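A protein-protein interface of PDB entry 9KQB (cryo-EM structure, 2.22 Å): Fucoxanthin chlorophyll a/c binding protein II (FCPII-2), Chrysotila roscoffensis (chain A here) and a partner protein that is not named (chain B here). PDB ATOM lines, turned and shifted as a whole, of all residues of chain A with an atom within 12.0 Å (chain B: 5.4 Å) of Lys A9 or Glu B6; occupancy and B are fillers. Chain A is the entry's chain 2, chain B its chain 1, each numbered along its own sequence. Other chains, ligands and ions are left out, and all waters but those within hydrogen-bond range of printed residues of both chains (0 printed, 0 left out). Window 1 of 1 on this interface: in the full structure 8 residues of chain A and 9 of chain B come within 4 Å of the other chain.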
ATOM      1  N   ALA A   8     -17.992  17.862 -16.920  1.00  0.00           N
ATOM      2  CA  ALA A   8     -17.139  18.159 -18.064  1.00  0.00           C
ATOM      3  C   ALA A   8     -16.309  16.942 -18.453  1.00  0.00           C
ATOM      4  O   ALA A   8     -16.198  16.602 -19.630  1.00  0.00           O
ATOM      5  CB  ALA A   8     -16.236  19.342 -17.759  1.00  0.00           C
ATOM      6  N   LYS A   9     -15.724  16.291 -17.452  1.00  0.00           N
ATOM      7  CA  LYS A   9     -14.899  15.112 -17.682  1.00  0.00           C
ATOM      8  C   LYS A   9     -15.788  13.881 -17.806  1.00  0.00           C
ATOM      9  O   LYS A   9     -16.700  13.681 -16.995  1.00  0.00           O
ATOM     10  CB  LYS A   9     -13.893  14.941 -16.547  1.00  0.00           C
ATOM     11  CG  LYS A   9     -12.759  15.950 -16.555  1.00  0.00           C
ATOM     12  CD  LYS A   9     -11.690  15.577 -15.539  1.00  0.00           C
ATOM     13  CE  LYS A   9     -10.310  15.538 -16.171  1.00  0.00           C
ATOM     14  NZ  LYS A   9     -10.232  16.373 -17.401  1.00  0.00           N
ATOM     15  N   GLY A  10     -15.526  13.060 -18.817  1.00  0.00           N
ATOM     16  CA  GLY A  10     -16.308  11.854 -19.030  1.00  0.00           C
ATOM     17  C   GLY A  10     -17.697  12.106 -19.575  1.00  0.00           C
ATOM     18  O   GLY A  10     -18.573  11.240 -19.454  1.00  0.00           O
ATOM     19  N   ARG A  11     -17.922  13.274 -20.171  1.00  0.00           N
ATOM     20  CA  ARG A  11     -19.216  13.600 -20.760  1.00  0.00           C
ATOM     21  C   ARG A  11     -19.159  13.869 -22.257  1.00  0.00           C
ATOM     22  O   ARG A  11     -20.218  13.938 -22.888  1.00  0.00           O
ATOM     23  CB  ARG A  11     -19.827  14.827 -20.067  1.00  0.00           C
ATOM     24  CG  ARG A  11     -19.946  14.732 -18.551  1.00  0.00           C
ATOM     25  CD  ARG A  11     -21.365  14.447 -18.078  1.00  0.00           C
ATOM     26  NE  ARG A  11     -21.935  13.229 -18.639  1.00  0.00           N
ATOM     27  CZ  ARG A  11     -23.213  12.890 -18.534  1.00  0.00           C
ATOM     28  NH1 ARG A  11     -24.100  13.699 -17.979  1.00  0.00           N
ATOM     29  NH2 ARG A  11     -23.610  11.705 -18.991  1.00  0.00           N
ATOM     30  N   GLY A  12     -17.974  14.025 -22.851  1.00  0.00           N
ATOM     31  CA  GLY A  12     -17.880  14.335 -24.266  1.00  0.00           C
ATOM     32  C   GLY A  12     -18.083  13.143 -25.176  1.00  0.00           C
ATOM     33  O   GLY A  12     -18.187  13.316 -26.394  1.00  0.00           O
ATOM     34  N   TRP A  13     -18.136  11.932 -24.614  1.00  0.00           N
ATOM     35  CA  TRP A  13     -18.406  10.755 -25.433  1.00  0.00           C
ATOM     36  C   TRP A  13     -19.854  10.724 -25.901  1.00  0.00           C
ATOM     37  O   TRP A  13     -20.174  10.039 -26.879  1.00  0.00           O
ATOM     38  CB  TRP A  13     -18.066   9.482 -24.654  1.00  0.00           C
ATOM     39  CG  TRP A  13     -18.948   9.238 -23.465  1.00  0.00           C
ATOM     40  CD1 TRP A  13     -18.723   9.645 -22.184  1.00  0.00           C
ATOM     41  CD2 TRP A  13     -20.189   8.521 -23.444  1.00  0.00           C
ATOM     42  NE1 TRP A  13     -19.748   9.234 -21.368  1.00  0.00           N
ATOM     43  CE2 TRP A  13     -20.662   8.542 -22.117  1.00  0.00           C
ATOM     44  CE3 TRP A  13     -20.950   7.867 -24.419  1.00  0.00           C
ATOM     45  CZ2 TRP A  13     -21.857   7.936 -21.742  1.00  0.00           C
ATOM     46  CZ3 TRP A  13     -22.137   7.267 -24.043  1.00  0.00           C
ATOM     47  CH2 TRP A  13     -22.578   7.304 -22.716  1.00  0.00           C
ATOM     48  N   LEU A  14     -20.741  11.440 -25.203  1.00  0.00           N
ATOM     49  CA  LEU A  14     -22.142  11.513 -25.606  1.00  0.00           C
ATOM     50  C   LEU A  14     -22.311  12.238 -26.930  1.00  0.00           C
ATOM     51  O   LEU A  14     -23.148  11.843 -27.750  1.00  0.00           O
ATOM     52  CB  LEU A  14     -22.964  12.225 -24.533  1.00  0.00           C
ATOM     53  CG  LEU A  14     -23.075  11.600 -23.147  1.00  0.00           C
ATOM     54  CD1 LEU A  14     -23.318  12.702 -22.140  1.00  0.00           C
ATOM     55  CD2 LEU A  14     -24.188  10.576 -23.104  1.00  0.00           C
ATOM     56  N   GLN A  15     -21.543  13.310 -27.145  1.00  0.00           N
ATOM     57  CA  GLN A  15     -21.671  14.094 -28.369  1.00  0.00           C
ATOM     58  C   GLN A  15     -21.237  13.291 -29.588  1.00  0.00           C
ATOM     59  O   GLN A  15     -21.834  13.415 -30.664  1.00  0.00           O
ATOM     60  CB  GLN A  15     -20.859  15.382 -28.249  1.00  0.00           C
ATOM     61  CG  GLN A  15     -21.646  16.550 -27.678  1.00  0.00           C
ATOM     62  CD  GLN A  15     -21.929  16.396 -26.195  1.00  0.00           C
ATOM     63  OE1 GLN A  15     -23.069  16.169 -25.790  1.00  0.00           O
ATOM     64  NE2 GLN A  15     -20.889  16.517 -25.379  1.00  0.00           N
ATOM     65  N   LYS A  16     -20.202  12.462 -29.442  1.00  0.00           N
ATOM     66  CA  LYS A  16     -19.801  11.592 -30.538  1.00  0.00           C
ATOM     67  C   LYS A  16     -20.758  10.424 -30.724  1.00  0.00           C
ATOM     68  O   LYS A  16     -20.924   9.950 -31.853  1.00  0.00           O
ATOM     69  CB  LYS A  16     -18.378  11.081 -30.310  1.00  0.00           C
ATOM     70  CG  LYS A  16     -17.315  12.146 -30.510  1.00  0.00           C
ATOM     71  CD  LYS A  16     -16.096  11.898 -29.642  1.00  0.00           C
ATOM     72  CE  LYS A  16     -15.521  13.207 -29.131  1.00  0.00           C
ATOM     73  NZ  LYS A  16     -14.741  13.920 -30.181  1.00  0.00           N
ATOM     74  N   TYR B   3     -16.628  19.335  -7.207  1.00  0.00           N
ATOM     75  CA  TYR B   3     -16.089  18.247  -8.016  1.00  0.00           C
ATOM     76  C   TYR B   3     -17.164  17.638  -8.898  1.00  0.00           C
ATOM     77  O   TYR B   3     -17.111  16.457  -9.241  1.00  0.00           O
ATOM     78  CB  TYR B   3     -15.460  17.182  -7.121  1.00  0.00           C
ATOM     79  CG  TYR B   3     -14.200  17.681  -6.470  1.00  0.00           C
ATOM     80  CD1 TYR B   3     -13.130  18.102  -7.244  1.00  0.00           C
ATOM     81  CD2 TYR B   3     -14.094  17.775  -5.090  1.00  0.00           C
ATOM     82  CE1 TYR B   3     -11.980  18.580  -6.666  1.00  0.00           C
ATOM     83  CE2 TYR B   3     -12.943  18.254  -4.500  1.00  0.00           C
ATOM     84  CZ  TYR B   3     -11.892  18.655  -5.296  1.00  0.00           C
ATOM     85  OH  TYR B   3     -10.744  19.135  -4.727  1.00  0.00           O
ATOM     86  N   GLU B   4     -18.145  18.466  -9.260  1.00  0.00           N
ATOM     87  CA  GLU B   4     -19.218  18.021 -10.139  1.00  0.00           C
ATOM     88  C   GLU B   4     -18.720  17.734 -11.547  1.00  0.00           C
ATOM     89  O   GLU B   4     -19.278  16.873 -12.232  1.00  0.00           O
ATOM     90  CB  GLU B   4     -20.328  19.070 -10.184  1.00  0.00           C
ATOM     91  CG  GLU B   4     -21.154  19.159  -8.914  1.00  0.00           C
ATOM     92  CD  GLU B   4     -20.594  20.158  -7.920  1.00  0.00           C
ATOM     93  OE1 GLU B   4     -19.931  21.122  -8.358  1.00  0.00           O
ATOM     94  OE2 GLU B   4     -20.817  19.979  -6.704  1.00  0.00           O
ATOM     95  N   ASN B   5     -17.692  18.446 -12.001  1.00  0.00           N
ATOM     96  CA  ASN B   5     -17.150  18.249 -13.345  1.00  0.00           C
ATOM     97  C   ASN B   5     -15.928  17.328 -13.309  1.00  0.00           C
ATOM     98  O   ASN B   5     -14.826  17.680 -13.730  1.00  0.00           O
ATOM     99  CB  ASN B   5     -16.818  19.596 -13.977  1.00  0.00           C
ATOM    100  CG  ASN B   5     -18.056  20.421 -14.266  1.00  0.00           C
ATOM    101  OD1 ASN B   5     -18.593  20.392 -15.373  1.00  0.00           O
ATOM    102  ND2 ASN B   5     -18.521  21.160 -13.265  1.00  0.00           N
ATOM    103  N   GLU B   6     -16.144  16.123 -12.788  1.00  0.00           N
ATOM    104  CA  GLU B   6     -15.114  15.098 -12.718  1.00  0.00           C
ATOM    105  C   GLU B   6     -15.668  13.787 -13.256  1.00  0.00           C
ATOM    106  O   GLU B   6     -16.845  13.689 -13.616  1.00  0.00           O
ATOM    107  CB  GLU B   6     -14.600  14.893 -11.283  1.00  0.00           C
ATOM    108  CG  GLU B   6     -14.059  16.146 -10.612  1.00  0.00           C
ATOM    109  CD  GLU B   6     -12.629  16.450 -11.012  1.00  0.00           C
ATOM    110  OE1 GLU B   6     -11.970  15.560 -11.588  1.00  0.00           O
ATOM    111  OE2 GLU B   6     -12.165  17.580 -10.753  1.00  0.00           O
ATOM    112  N   LEU B   7     -14.799  12.780 -13.324  1.00  0.00           N
ATOM    113  CA  LEU B   7     -15.220  11.448 -13.737  1.00  0.00           C
ATOM    114  C   LEU B   7     -16.153  10.838 -12.702  1.00  0.00           C
ATOM    115  O   LEU B   7     -16.072  11.146 -11.510  1.00  0.00           O
ATOM    116  CB  LEU B   7     -14.005  10.542 -13.939  1.00  0.00           C
ATOM    117  CG  LEU B   7     -13.088  10.739 -15.145  1.00  0.00           C
ATOM    118  CD1 LEU B   7     -12.484   9.412 -15.523  1.00  0.00           C
ATOM    119  CD2 LEU B   7     -13.849  11.296 -16.323  1.00  0.00           C
ATOM    120  N   GLY B   8     -17.044   9.965 -13.163  1.00  0.00           N
ATOM    121  CA  GLY B   8     -17.990   9.290 -12.299  1.00  0.00           C
ATOM    122  C   GLY B   8     -19.386   9.868 -12.312  1.00  0.00           C
ATOM    123  O   GLY B   8     -20.287   9.278 -11.702  1.00  0.00           O
ATOM    124  N   VAL B   9     -19.599  11.001 -12.973  1.00  0.00           N
ATOM    125  CA  VAL B   9     -20.934  11.573 -13.102  1.00  0.00           C
ATOM    126  C   VAL B   9     -21.636  10.884 -14.265  1.00  0.00           C
ATOM    127  O   VAL B   9     -21.171  10.947 -15.408  1.00  0.00           O
ATOM    128  CB  VAL B   9     -20.868  13.091 -13.307  1.00  0.00           C
ATOM    129  CG1 VAL B   9     -22.243  13.707 -13.149  1.00  0.00           C
ATOM    130  CG2 VAL B   9     -19.907  13.694 -12.311  1.00  0.00           C
ATOM    131  N   PHE B  30      -9.485  14.030  -2.725  1.00  0.00           N
ATOM    132  CA  PHE B  30     -10.348  13.547  -3.801  1.00  0.00           C
ATOM    133  C   PHE B  30      -9.615  12.558  -4.693  1.00  0.00           C
ATOM    134  O   PHE B  30     -10.205  11.573  -5.152  1.00  0.00           O
ATOM    135  CB  PHE B  30     -10.877  14.705  -4.645  1.00  0.00           C
ATOM    136  CG  PHE B  30     -11.836  14.268  -5.719  1.00  0.00           C
ATOM    137  CD1 PHE B  30     -13.129  13.885  -5.398  1.00  0.00           C
ATOM    138  CD2 PHE B  30     -11.435  14.210  -7.046  1.00  0.00           C
ATOM    139  CE1 PHE B  30     -14.010  13.471  -6.381  1.00  0.00           C
ATOM    140  CE2 PHE B  30     -12.312  13.795  -8.034  1.00  0.00           C
ATOM    141  CZ  PHE B  30     -13.600  13.426  -7.700  1.00  0.00           C
ATOM    142  N   ARG B  34     -10.871   8.843  -5.216  1.00  0.00           N
ATOM    143  CA  ARG B  34     -11.090   8.176  -6.495  1.00  0.00           C
ATOM    144  C   ARG B  34     -10.181   6.960  -6.639  1.00  0.00           C
ATOM    145  O   ARG B  34     -10.588   5.932  -7.193  1.00  0.00           O
ATOM    146  CB  ARG B  34     -10.885   9.173  -7.641  1.00  0.00           C
ATOM    147  CG  ARG B  34     -10.714   8.572  -9.038  1.00  0.00           C
ATOM    148  CD  ARG B  34     -11.945   7.811  -9.537  1.00  0.00           C
ATOM    149  NE  ARG B  34     -13.209   8.349  -9.046  1.00  0.00           N
ATOM    150  CZ  ARG B  34     -13.874   9.342  -9.617  1.00  0.00           C
ATOM    151  NH1 ARG B  34     -13.415   9.950 -10.698  1.00  0.00           N
ATOM    152  NH2 ARG B  34     -15.029   9.736  -9.090  1.00  0.00           N
ATOM    153  N   GLU B 119     -11.961   8.268 -21.426  1.00  0.00           N
ATOM    154  CA  GLU B 119     -12.777   8.702 -20.295  1.00  0.00           C
ATOM    155  C   GLU B 119     -14.094   7.940 -20.235  1.00  0.00           C
ATOM    156  O   GLU B 119     -14.626   7.705 -19.145  1.00  0.00           O
ATOM    157  CB  GLU B 119     -13.038  10.208 -20.353  1.00  0.00           C
ATOM    158  CG  GLU B 119     -11.816  11.061 -20.624  1.00  0.00           C
ATOM    159  CD  GLU B 119     -12.038  12.523 -20.289  1.00  0.00           C
ATOM    160  OE1 GLU B 119     -11.390  13.385 -20.920  1.00  0.00           O
ATOM    161  OE2 GLU B 119     -12.861  12.811 -19.395  1.00  0.00           O
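The side-chain carboxylate of Glu B119 lies within hydrogen-bond range of the backbone NH of Gly A10 (2.7 Å).
O of Glu B6 lies close to O of Lys A9 (3.4 Å).
The side-chain amide oxygen of Asn B5 lies within hydrogen-bond range of the backbone NH of Ala A8 (3.0 Å).
The backbone carbonyl oxygen (O) of Gly A10 is in hydrogen-bond range of the indole nitrogen (NE1) of Trp A13, at 3.0 Å.
The backbone carbonyl oxygen of Leu B7 sits at hydrogen-bond distance from the guanidinium group of Arg B34 (3.0 Å).
Among the printed residues, pairs that only touch across the chains: Gly A10 with Leu B7, Lys A9 with Glu B119, Lys A9 with Leu B7 and Lys A9 with Asn B5.
Of chain B, only Asn B5, Glu B6, Leu B7 and Glu B119 come within 4 Å of Lys A9.
Of chain A, only Lys A9 (3.4 Å) comes within 4 Å of Glu B6.
No residue of chain A comes within 4 Å of Tyr B3.
Leu B7 touches just these residues of chain A: Lys A9 and Gly A10.
Gly B8 touches none of the printed residues of chain A.
No residue of chain A comes within 4 Å of Val B9.
Printed residues of chain A within 4 Å of Glu B119: Lys A9 (3.5 Å) and Gly A10 (2.7 Å).
Printed residues of chain B within 4 Å of Ala A8: Asn B5.
Printed residues of chain B within 4 Å of Gly A10: Leu B7 (3.5 Å) and Glu B119 (2.7 Å).
Leu A14 touches none of the printed residues of chain B.
Lys A16 touches none of the printed residues of chain B.
The nearest residue of chain A that does not touch Glu B6 is Ala A8 (4.8 Å).
The nearest printed residue of chain B that does not touch Gly A10 is Val B9 (4.8 Å).
Hydrophobic or aromatic side chains of chain A that line the printed part of chain B: Ala A8.
Of the 10 printed residues of chain B, 4 touch a printed residue of chain A.
Among the printed residues, no Asp or Glu carboxylate lies within 4 Å of a Lys or Arg side-chain nitrogen of the other chain.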
